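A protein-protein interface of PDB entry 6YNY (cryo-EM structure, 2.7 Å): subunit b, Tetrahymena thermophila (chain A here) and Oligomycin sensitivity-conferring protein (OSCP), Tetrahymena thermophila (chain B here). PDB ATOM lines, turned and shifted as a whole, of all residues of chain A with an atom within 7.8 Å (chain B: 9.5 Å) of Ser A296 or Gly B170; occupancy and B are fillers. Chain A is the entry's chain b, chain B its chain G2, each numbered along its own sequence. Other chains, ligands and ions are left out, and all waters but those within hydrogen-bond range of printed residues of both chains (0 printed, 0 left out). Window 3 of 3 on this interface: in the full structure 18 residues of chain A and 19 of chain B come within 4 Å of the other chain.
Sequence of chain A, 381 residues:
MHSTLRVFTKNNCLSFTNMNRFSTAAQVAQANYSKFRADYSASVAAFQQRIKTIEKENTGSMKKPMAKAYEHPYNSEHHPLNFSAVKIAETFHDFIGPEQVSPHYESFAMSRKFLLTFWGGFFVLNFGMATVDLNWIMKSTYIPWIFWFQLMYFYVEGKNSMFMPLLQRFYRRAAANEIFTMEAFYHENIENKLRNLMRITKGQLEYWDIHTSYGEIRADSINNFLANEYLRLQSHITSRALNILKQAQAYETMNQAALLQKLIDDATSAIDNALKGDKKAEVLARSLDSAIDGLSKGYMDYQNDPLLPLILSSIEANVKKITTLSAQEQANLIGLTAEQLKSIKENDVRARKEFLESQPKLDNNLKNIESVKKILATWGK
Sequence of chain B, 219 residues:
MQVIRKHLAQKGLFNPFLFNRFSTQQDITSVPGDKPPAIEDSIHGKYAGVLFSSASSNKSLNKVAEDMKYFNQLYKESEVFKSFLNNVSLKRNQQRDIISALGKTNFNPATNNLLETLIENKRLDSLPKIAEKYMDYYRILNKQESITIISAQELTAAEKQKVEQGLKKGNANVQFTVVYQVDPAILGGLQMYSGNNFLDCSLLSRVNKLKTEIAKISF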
ATOM      1  N   ASP A 289      -5.962  16.135 -10.397  1.00  0.00           N
ATOM      2  CA  ASP A 289      -5.605  14.828 -10.941  1.00  0.00           C
ATOM      3  C   ASP A 289      -5.859  13.729  -9.917  1.00  0.00           C
ATOM      4  O   ASP A 289      -6.463  12.696 -10.231  1.00  0.00           O
ATOM      5  CB  ASP A 289      -4.141  14.830 -11.381  1.00  0.00           C
ATOM      6  CG  ASP A 289      -3.736  13.539 -12.067  1.00  0.00           C
ATOM      7  OD1 ASP A 289      -4.614  12.679 -12.293  1.00  0.00           O
ATOM      8  OD2 ASP A 289      -2.537  13.382 -12.380  1.00  0.00           O
ATOM      9  N   SER A 290      -5.402  13.936  -8.680  1.00  0.00           N
ATOM     10  CA  SER A 290      -5.647  12.955  -7.631  1.00  0.00           C
ATOM     11  C   SER A 290      -7.130  12.850  -7.298  1.00  0.00           C
ATOM     12  O   SER A 290      -7.586  11.802  -6.826  1.00  0.00           O
ATOM     13  CB  SER A 290      -4.847  13.316  -6.379  1.00  0.00           C
ATOM     14  OG  SER A 290      -5.069  12.375  -5.343  1.00  0.00           O
ATOM     15  N   ALA A 291      -7.895  13.918  -7.534  1.00  0.00           N
ATOM     16  CA  ALA A 291      -9.327  13.878  -7.252  1.00  0.00           C
ATOM     17  C   ALA A 291     -10.052  12.961  -8.228  1.00  0.00           C
ATOM     18  O   ALA A 291     -10.779  12.050  -7.816  1.00  0.00           O
ATOM     19  CB  ALA A 291      -9.909  15.290  -7.305  1.00  0.00           C
ATOM     20  N   ILE A 292      -9.865  13.185  -9.532  1.00  0.00           N
ATOM     21  CA  ILE A 292     -10.526  12.351 -10.530  1.00  0.00           C
ATOM     22  C   ILE A 292     -10.149  10.890 -10.343  1.00  0.00           C
ATOM     23  O   ILE A 292     -10.968   9.992 -10.578  1.00  0.00           O
ATOM     24  CB  ILE A 292     -10.190  12.848 -11.951  1.00  0.00           C
ATOM     25  CG1 ILE A 292     -11.114  14.004 -12.347  1.00  0.00           C
ATOM     26  CG2 ILE A 292     -10.309  11.717 -12.967  1.00  0.00           C
ATOM     27  CD1 ILE A 292     -10.966  15.243 -11.491  1.00  0.00           C
ATOM     28  N   ASP A 293      -8.912  10.621  -9.922  1.00  0.00           N
ATOM     29  CA  ASP A 293      -8.498   9.243  -9.675  1.00  0.00           C
ATOM     30  C   ASP A 293      -9.391   8.590  -8.628  1.00  0.00           C
ATOM     31  O   ASP A 293      -9.841   7.451  -8.800  1.00  0.00           O
ATOM     32  CB  ASP A 293      -7.034   9.210  -9.234  1.00  0.00           C
ATOM     33  CG  ASP A 293      -6.547   7.804  -8.941  1.00  0.00           C
ATOM     34  OD1 ASP A 293      -6.408   7.010  -9.894  1.00  0.00           O
ATOM     35  OD2 ASP A 293      -6.304   7.494  -7.756  1.00  0.00           O
ATOM     36  N   GLY A 294      -9.657   9.299  -7.531  1.00  0.00           N
ATOM     37  CA  GLY A 294     -10.541   8.757  -6.512  1.00  0.00           C
ATOM     38  C   GLY A 294     -11.959   8.568  -7.013  1.00  0.00           C
ATOM     39  O   GLY A 294     -12.598   7.552  -6.729  1.00  0.00           O
ATOM     40  N   LEU A 295     -12.474   9.546  -7.763  1.00  0.00           N
ATOM     41  CA  LEU A 295     -13.835   9.439  -8.279  1.00  0.00           C
ATOM     42  C   LEU A 295     -13.987   8.217  -9.174  1.00  0.00           C
ATOM     43  O   LEU A 295     -14.978   7.484  -9.077  1.00  0.00           O
ATOM     44  CB  LEU A 295     -14.205  10.710  -9.043  1.00  0.00           C
ATOM     45  CG  LEU A 295     -14.071  12.030  -8.280  1.00  0.00           C
ATOM     46  CD1 LEU A 295     -14.414  13.203  -9.185  1.00  0.00           C
ATOM     47  CD2 LEU A 295     -14.950  12.038  -7.041  1.00  0.00           C
ATOM     48  N   SER A 296     -13.012   7.980 -10.055  1.00  0.00           N
ATOM     49  CA  SER A 296     -13.083   6.827 -10.945  1.00  0.00           C
ATOM     50  C   SER A 296     -13.046   5.517 -10.170  1.00  0.00           C
ATOM     51  O   SER A 296     -13.563   4.500 -10.645  1.00  0.00           O
ATOM     52  CB  SER A 296     -11.937   6.875 -11.955  1.00  0.00           C
ATOM     53  OG  SER A 296     -10.680   6.847 -11.301  1.00  0.00           O
ATOM     54  N   LYS A 297     -12.443   5.521  -8.987  1.00  0.00           N
ATOM     55  CA  LYS A 297     -12.321   4.333  -8.157  1.00  0.00           C
ATOM     56  C   LYS A 297     -13.369   4.350  -7.049  1.00  0.00           C
ATOM     57  O   LYS A 297     -13.981   5.378  -6.752  1.00  0.00           O
ATOM     58  CB  LYS A 297     -10.913   4.248  -7.560  1.00  0.00           C
ATOM     59  CG  LYS A 297     -10.623   2.967  -6.795  1.00  0.00           C
ATOM     60  CD  LYS A 297      -9.127   2.756  -6.607  1.00  0.00           C
ATOM     61  CE  LYS A 297      -8.475   3.933  -5.894  1.00  0.00           C
ATOM     62  NZ  LYS A 297      -7.038   3.678  -5.599  1.00  0.00           N
ATOM     63  N   GLY A 298     -13.574   3.181  -6.438  1.00  0.00           N
ATOM     64  CA  GLY A 298     -14.581   3.074  -5.396  1.00  0.00           C
ATOM     65  C   GLY A 298     -14.264   3.931  -4.185  1.00  0.00           C
ATOM     66  O   GLY A 298     -15.165   4.484  -3.552  1.00  0.00           O
ATOM     67  N   TYR A 299     -12.985   4.051  -3.848  1.00  0.00           N
ATOM     68  CA  TYR A 299     -12.528   4.835  -2.711  1.00  0.00           C
ATOM     69  C   TYR A 299     -11.594   5.941  -3.197  1.00  0.00           C
ATOM     70  O   TYR A 299     -11.392   6.134  -4.398  1.00  0.00           O
ATOM     71  CB  TYR A 299     -11.836   3.940  -1.678  1.00  0.00           C
ATOM     72  CG  TYR A 299     -10.658   3.166  -2.223  1.00  0.00           C
ATOM     73  CD1 TYR A 299     -10.837   1.933  -2.835  1.00  0.00           C
ATOM     74  CD2 TYR A 299      -9.367   3.666  -2.123  1.00  0.00           C
ATOM     75  CE1 TYR A 299      -9.763   1.220  -3.333  1.00  0.00           C
ATOM     76  CE2 TYR A 299      -8.287   2.961  -2.618  1.00  0.00           C
ATOM     77  CZ  TYR A 299      -8.491   1.739  -3.222  1.00  0.00           C
ATOM     78  OH  TYR A 299      -7.418   1.033  -3.717  1.00  0.00           O
ATOM     79  N   ILE B 147     -25.940  13.546 -10.454  1.00  0.00           N
ATOM     80  CA  ILE B 147     -24.687  13.621  -9.712  1.00  0.00           C
ATOM     81  C   ILE B 147     -24.239  15.075  -9.684  1.00  0.00           C
ATOM     82  O   ILE B 147     -24.162  15.729 -10.731  1.00  0.00           O
ATOM     83  CB  ILE B 147     -23.605  12.723 -10.341  1.00  0.00           C
ATOM     84  CG1 ILE B 147     -24.085  11.271 -10.387  1.00  0.00           C
ATOM     85  CG2 ILE B 147     -22.304  12.833  -9.552  1.00  0.00           C
ATOM     86  CD1 ILE B 147     -23.148  10.331 -11.122  1.00  0.00           C
ATOM     87  N   LYS B 162     -12.896  15.545 -18.674  1.00  0.00           N
ATOM     88  CA  LYS B 162     -12.184  14.501 -17.946  1.00  0.00           C
ATOM     89  C   LYS B 162     -13.002  13.992 -16.768  1.00  0.00           C
ATOM     90  O   LYS B 162     -12.919  12.809 -16.418  1.00  0.00           O
ATOM     91  CB  LYS B 162     -10.831  15.029 -17.469  1.00  0.00           C
ATOM     92  CG  LYS B 162      -9.922  15.489 -18.595  1.00  0.00           C
ATOM     93  CD  LYS B 162      -8.604  16.028 -18.065  1.00  0.00           C
ATOM     94  CE  LYS B 162      -7.700  16.496 -19.195  1.00  0.00           C
ATOM     95  NZ  LYS B 162      -7.341  15.388 -20.123  1.00  0.00           N
ATOM     96  N   VAL B 163     -13.796  14.866 -16.145  1.00  0.00           N
ATOM     97  CA  VAL B 163     -14.630  14.443 -15.024  1.00  0.00           C
ATOM     98  C   VAL B 163     -15.656  13.419 -15.487  1.00  0.00           C
ATOM     99  O   VAL B 163     -15.986  12.474 -14.758  1.00  0.00           O
ATOM    100  CB  VAL B 163     -15.305  15.664 -14.372  1.00  0.00           C
ATOM    101  CG1 VAL B 163     -16.288  15.221 -13.298  1.00  0.00           C
ATOM    102  CG2 VAL B 163     -14.259  16.602 -13.790  1.00  0.00           C
ATOM    103  N   GLU B 164     -16.178  13.584 -16.705  1.00  0.00           N
ATOM    104  CA  GLU B 164     -17.175  12.646 -17.210  1.00  0.00           C
ATOM    105  C   GLU B 164     -16.583  11.253 -17.374  1.00  0.00           C
ATOM    106  O   GLU B 164     -17.215  10.254 -17.009  1.00  0.00           O
ATOM    107  CB  GLU B 164     -17.740  13.143 -18.541  1.00  0.00           C
ATOM    108  CG  GLU B 164     -18.187  14.597 -18.534  1.00  0.00           C
ATOM    109  CD  GLU B 164     -19.167  14.905 -17.420  1.00  0.00           C
ATOM    110  OE1 GLU B 164     -19.835  13.964 -16.940  1.00  0.00           O
ATOM    111  OE2 GLU B 164     -19.268  16.084 -17.024  1.00  0.00           O
ATOM    112  N   GLN B 165     -15.369  11.163 -17.922  1.00  0.00           N
ATOM    113  CA  GLN B 165     -14.740   9.859 -18.102  1.00  0.00           C
ATOM    114  C   GLN B 165     -14.487   9.184 -16.761  1.00  0.00           C
ATOM    115  O   GLN B 165     -14.595   7.957 -16.645  1.00  0.00           O
ATOM    116  CB  GLN B 165     -13.434  10.011 -18.881  1.00  0.00           C
ATOM    117  CG  GLN B 165     -13.577  10.754 -20.202  1.00  0.00           C
ATOM    118  CD  GLN B 165     -14.635  10.150 -21.110  1.00  0.00           C
ATOM    119  OE1 GLN B 165     -15.346  10.868 -21.812  1.00  0.00           O
ATOM    120  NE2 GLN B 165     -14.738   8.824 -21.105  1.00  0.00           N
ATOM    121  N   GLY B 166     -14.147   9.967 -15.737  1.00  0.00           N
ATOM    122  CA  GLY B 166     -13.931   9.385 -14.422  1.00  0.00           C
ATOM    123  C   GLY B 166     -15.211   8.840 -13.817  1.00  0.00           C
ATOM    124  O   GLY B 166     -15.253   7.702 -13.341  1.00  0.00           O
ATOM    125  N   LEU B 167     -16.275   9.645 -13.830  1.00  0.00           N
ATOM    126  CA  LEU B 167     -17.557   9.176 -13.316  1.00  0.00           C
ATOM    127  C   LEU B 167     -18.085   8.013 -14.143  1.00  0.00           C
ATOM    128  O   LEU B 167     -18.627   7.045 -13.597  1.00  0.00           O
ATOM    129  CB  LEU B 167     -18.566  10.324 -13.305  1.00  0.00           C
ATOM    130  CG  LEU B 167     -18.173  11.557 -12.489  1.00  0.00           C
ATOM    131  CD1 LEU B 167     -19.204  12.659 -12.664  1.00  0.00           C
ATOM    132  CD2 LEU B 167     -18.007  11.206 -11.019  1.00  0.00           C
ATOM    133  N   LYS B 168     -17.937   8.090 -15.467  1.00  0.00           N
ATOM    134  CA  LYS B 168     -18.388   7.004 -16.331  1.00  0.00           C
ATOM    135  C   LYS B 168     -17.636   5.715 -16.022  1.00  0.00           C
ATOM    136  O   LYS B 168     -18.245   4.666 -15.786  1.00  0.00           O
ATOM    137  CB  LYS B 168     -18.211   7.398 -17.798  1.00  0.00           C
ATOM    138  CG  LYS B 168     -18.599   6.311 -18.796  1.00  0.00           C
ATOM    139  CD  LYS B 168     -20.040   5.844 -18.617  1.00  0.00           C
ATOM    140  CE  LYS B 168     -21.037   6.973 -18.832  1.00  0.00           C
ATOM    141  NZ  LYS B 168     -22.444   6.496 -18.755  1.00  0.00           N
ATOM    142  N   LYS B 169     -16.302   5.778 -16.021  1.00  0.00           N
ATOM    143  CA  LYS B 169     -15.507   4.592 -15.725  1.00  0.00           C
ATOM    144  C   LYS B 169     -15.781   4.065 -14.323  1.00  0.00           C
ATOM    145  O   LYS B 169     -15.646   2.861 -14.077  1.00  0.00           O
ATOM    146  CB  LYS B 169     -14.020   4.907 -15.889  1.00  0.00           C
ATOM    147  CG  LYS B 169     -13.106   3.717 -15.637  1.00  0.00           C
ATOM    148  CD  LYS B 169     -11.673   4.005 -16.063  1.00  0.00           C
ATOM    149  CE  LYS B 169     -11.053   5.125 -15.242  1.00  0.00           C
ATOM    150  NZ  LYS B 169      -9.639   5.384 -15.631  1.00  0.00           N
ATOM    151  N   GLY B 170     -16.164   4.938 -13.395  1.00  0.00           N
ATOM    152  CA  GLY B 170     -16.487   4.501 -12.052  1.00  0.00           C
ATOM    153  C   GLY B 170     -17.695   3.589 -12.027  1.00  0.00           C
ATOM    154  O   GLY B 170     -17.623   2.467 -11.517  1.00  0.00           O
ATOM    155  N   ASN B 171     -18.815   4.061 -12.577  1.00  0.00           N
ATOM    156  CA  ASN B 171     -20.011   3.231 -12.662  1.00  0.00           C
ATOM    157  C   ASN B 171     -19.934   2.289 -13.859  1.00  0.00           C
ATOM    158  O   ASN B 171     -19.923   1.064 -13.702  1.00  0.00           O
ATOM    159  CB  ASN B 171     -21.257   4.116 -12.751  1.00  0.00           C
ATOM    160  CG  ASN B 171     -21.373   5.080 -11.589  1.00  0.00           C
ATOM    161  OD1 ASN B 171     -20.942   4.783 -10.475  1.00  0.00           O
ATOM    162  ND2 ASN B 171     -21.957   6.245 -11.843  1.00  0.00           N
ATOM    163  N   ALA B 172     -19.883   2.853 -15.063  1.00  0.00           N
ATOM    164  CA  ALA B 172     -19.743   2.122 -16.317  1.00  0.00           C
ATOM    165  C   ALA B 172     -20.910   1.182 -16.593  1.00  0.00           C
ATOM    166  O   ALA B 172     -20.843   0.381 -17.534  1.00  0.00           O
ATOM    167  CB  ALA B 172     -18.429   1.330 -16.353  1.00  0.00           C
ATOM    168  N   ASN B 173     -21.983   1.251 -15.800  1.00  0.00           N
ATOM    169  CA  ASN B 173     -23.132   0.383 -16.008  1.00  0.00           C
ATOM    170  C   ASN B 173     -24.470   1.088 -15.835  1.00  0.00           C
ATOM    171  O   ASN B 173     -25.507   0.422 -15.917  1.00  0.00           O
ATOM    172  CB  ASN B 173     -23.069  -0.816 -15.046  1.00  0.00           C
ATOM    173  CG  ASN B 173     -21.822  -1.655 -15.241  1.00  0.00           C
ATOM    174  OD1 ASN B 173     -21.822  -2.622 -16.003  1.00  0.00           O
ATOM    175  ND2 ASN B 173     -20.747  -1.287 -14.552  1.00  0.00           N
ATOM    176  N   VAL B 174     -24.487   2.397 -15.600  1.00  0.00           N
ATOM    177  CA  VAL B 174     -25.731   3.137 -15.412  1.00  0.00           C
ATOM    178  C   VAL B 174     -25.549   4.537 -15.978  1.00  0.00           C
ATOM    179  O   VAL B 174     -24.534   5.192 -15.720  1.00  0.00           O
ATOM    180  CB  VAL B 174     -26.147   3.203 -13.926  1.00  0.00           C
ATOM    181  CG1 VAL B 174     -26.407   1.806 -13.383  1.00  0.00           C
ATOM    182  CG2 VAL B 174     -25.083   3.914 -13.102  1.00  0.00           C
ATOM    183  N   PHE B 176     -26.317   8.546 -16.256  1.00  0.00           N
ATOM    184  CA  PHE B 176     -26.533   9.557 -15.232  1.00  0.00           C
ATOM    185  C   PHE B 176     -26.440  10.940 -15.858  1.00  0.00           C
ATOM    186  O   PHE B 176     -25.847  11.125 -16.923  1.00  0.00           O
ATOM    187  CB  PHE B 176     -25.518   9.423 -14.090  1.00  0.00           C
ATOM    188  CG  PHE B 176     -24.088   9.412 -14.549  1.00  0.00           C
ATOM    189  CD1 PHE B 176     -23.394  10.598 -14.725  1.00  0.00           C
ATOM    190  CD2 PHE B 176     -23.438   8.216 -14.804  1.00  0.00           C
ATOM    191  CE1 PHE B 176     -22.078  10.591 -15.147  1.00  0.00           C
ATOM    192  CE2 PHE B 176     -22.122   8.203 -15.227  1.00  0.00           C
ATOM    193  CZ  PHE B 176     -21.441   9.392 -15.398  1.00  0.00           C
ATOM    194  N   MET B 192     -18.461  14.931  -4.440  1.00  0.00           N
ATOM    195  CA  MET B 192     -19.527  14.453  -5.307  1.00  0.00           C
ATOM    196  C   MET B 192     -20.728  14.029  -4.472  1.00  0.00           C
ATOM    197  O   MET B 192     -20.576  13.392  -3.424  1.00  0.00           O
ATOM    198  CB  MET B 192     -19.051  13.277  -6.165  1.00  0.00           C
ATOM    199  CG  MET B 192     -18.582  12.066  -5.366  1.00  0.00           C
ATOM    200  SD  MET B 192     -18.206  10.636  -6.397  1.00  0.00           S
ATOM    201  CE  MET B 192     -19.819  10.265  -7.081  1.00  0.00           C
ATOM    202  N   LEU B 199     -18.774  11.014  -1.613  1.00  0.00           N
ATOM    203  CA  LEU B 199     -17.364  10.644  -1.659  1.00  0.00           C
ATOM    204  C   LEU B 199     -16.548  11.926  -1.643  1.00  0.00           C
ATOM    205  O   LEU B 199     -16.731  12.790  -2.506  1.00  0.00           O
ATOM    206  CB  LEU B 199     -17.051   9.811  -2.906  1.00  0.00           C
ATOM    207  CG  LEU B 199     -15.735   9.024  -2.937  1.00  0.00           C
ATOM    208  CD1 LEU B 199     -14.531   9.953  -2.922  1.00  0.00           C
ATOM    209  CD2 LEU B 199     -15.664   8.036  -1.781  1.00  0.00           C
ATOM    210  N   CYS B 201     -13.198  13.875  -2.101  1.00  0.00           N
ATOM    211  CA  CYS B 201     -11.865  13.972  -2.681  1.00  0.00           C
ATOM    212  C   CYS B 201     -11.237  15.337  -2.424  1.00  0.00           C
ATOM    213  O   CYS B 201     -10.274  15.712  -3.101  1.00  0.00           O
ATOM    214  CB  CYS B 201     -11.916  13.691  -4.184  1.00  0.00           C
ATOM    215  SG  CYS B 201     -12.545  12.056  -4.621  1.00  0.00           S
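The side-chain sulfur (SG) of Cys B201 sits at hydrogen-bond distance from the backbone carbonyl oxygen (O) of Ala A291, at 3.7 Å.
The backbone carbonyl oxygen of Ile A292 lies within hydrogen-bond range of the side-chain hydroxyl of Ser A296, 3.2 Å away. OG of Ser A296 sits at hydrogen-bond distance from O of Asp A293 (2.7 Å). The backbone NH (N) of Met B192 is in hydrogen-bond range of the backbone carbonyl oxygen (O) of Leu B199 (3.4 Å).
Among the printed residues, merely in contact across the chains: Leu A295 with Met B192 (3.6 Å), Leu A295 with Cys B201 (3.4 Å), Ser A296 with Gly B166 (3.3 Å), Ser A296 with Lys B169 (3.8 Å) and Ser A296 with Gly B170 (3.2 Å).
Ser A296 touches three residues of chain B. Gly B170 touches just one residue of chain A: Ser A296 (3.2 Å). No residue of chain B comes within 4 Å of Gly A294. Of the printed residues of chain A, Met B192 touches Leu A295 (3.6 Å). Printed residues of chain A within 4 Å of Cys B201: Ala A291 and Leu A295. Printed residues of chain A within 4 Å of Lys B169: Ser A296. Printed residues of chain B within 4 Å of Leu A295: Met B192 (3.6 Å) and Cys B201 (3.4 Å). The nearest residue of chain B that does not touch Ser A296 is Leu B167 (5.1 Å).
Of the 11 printed residues of chain A, 3 touch a printed residue of chain B. Hydrophobic or aromatic side chains of chain B that line the printed part of chain A: Met B192. Among the printed residues, 6 pairs touch across the chains.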
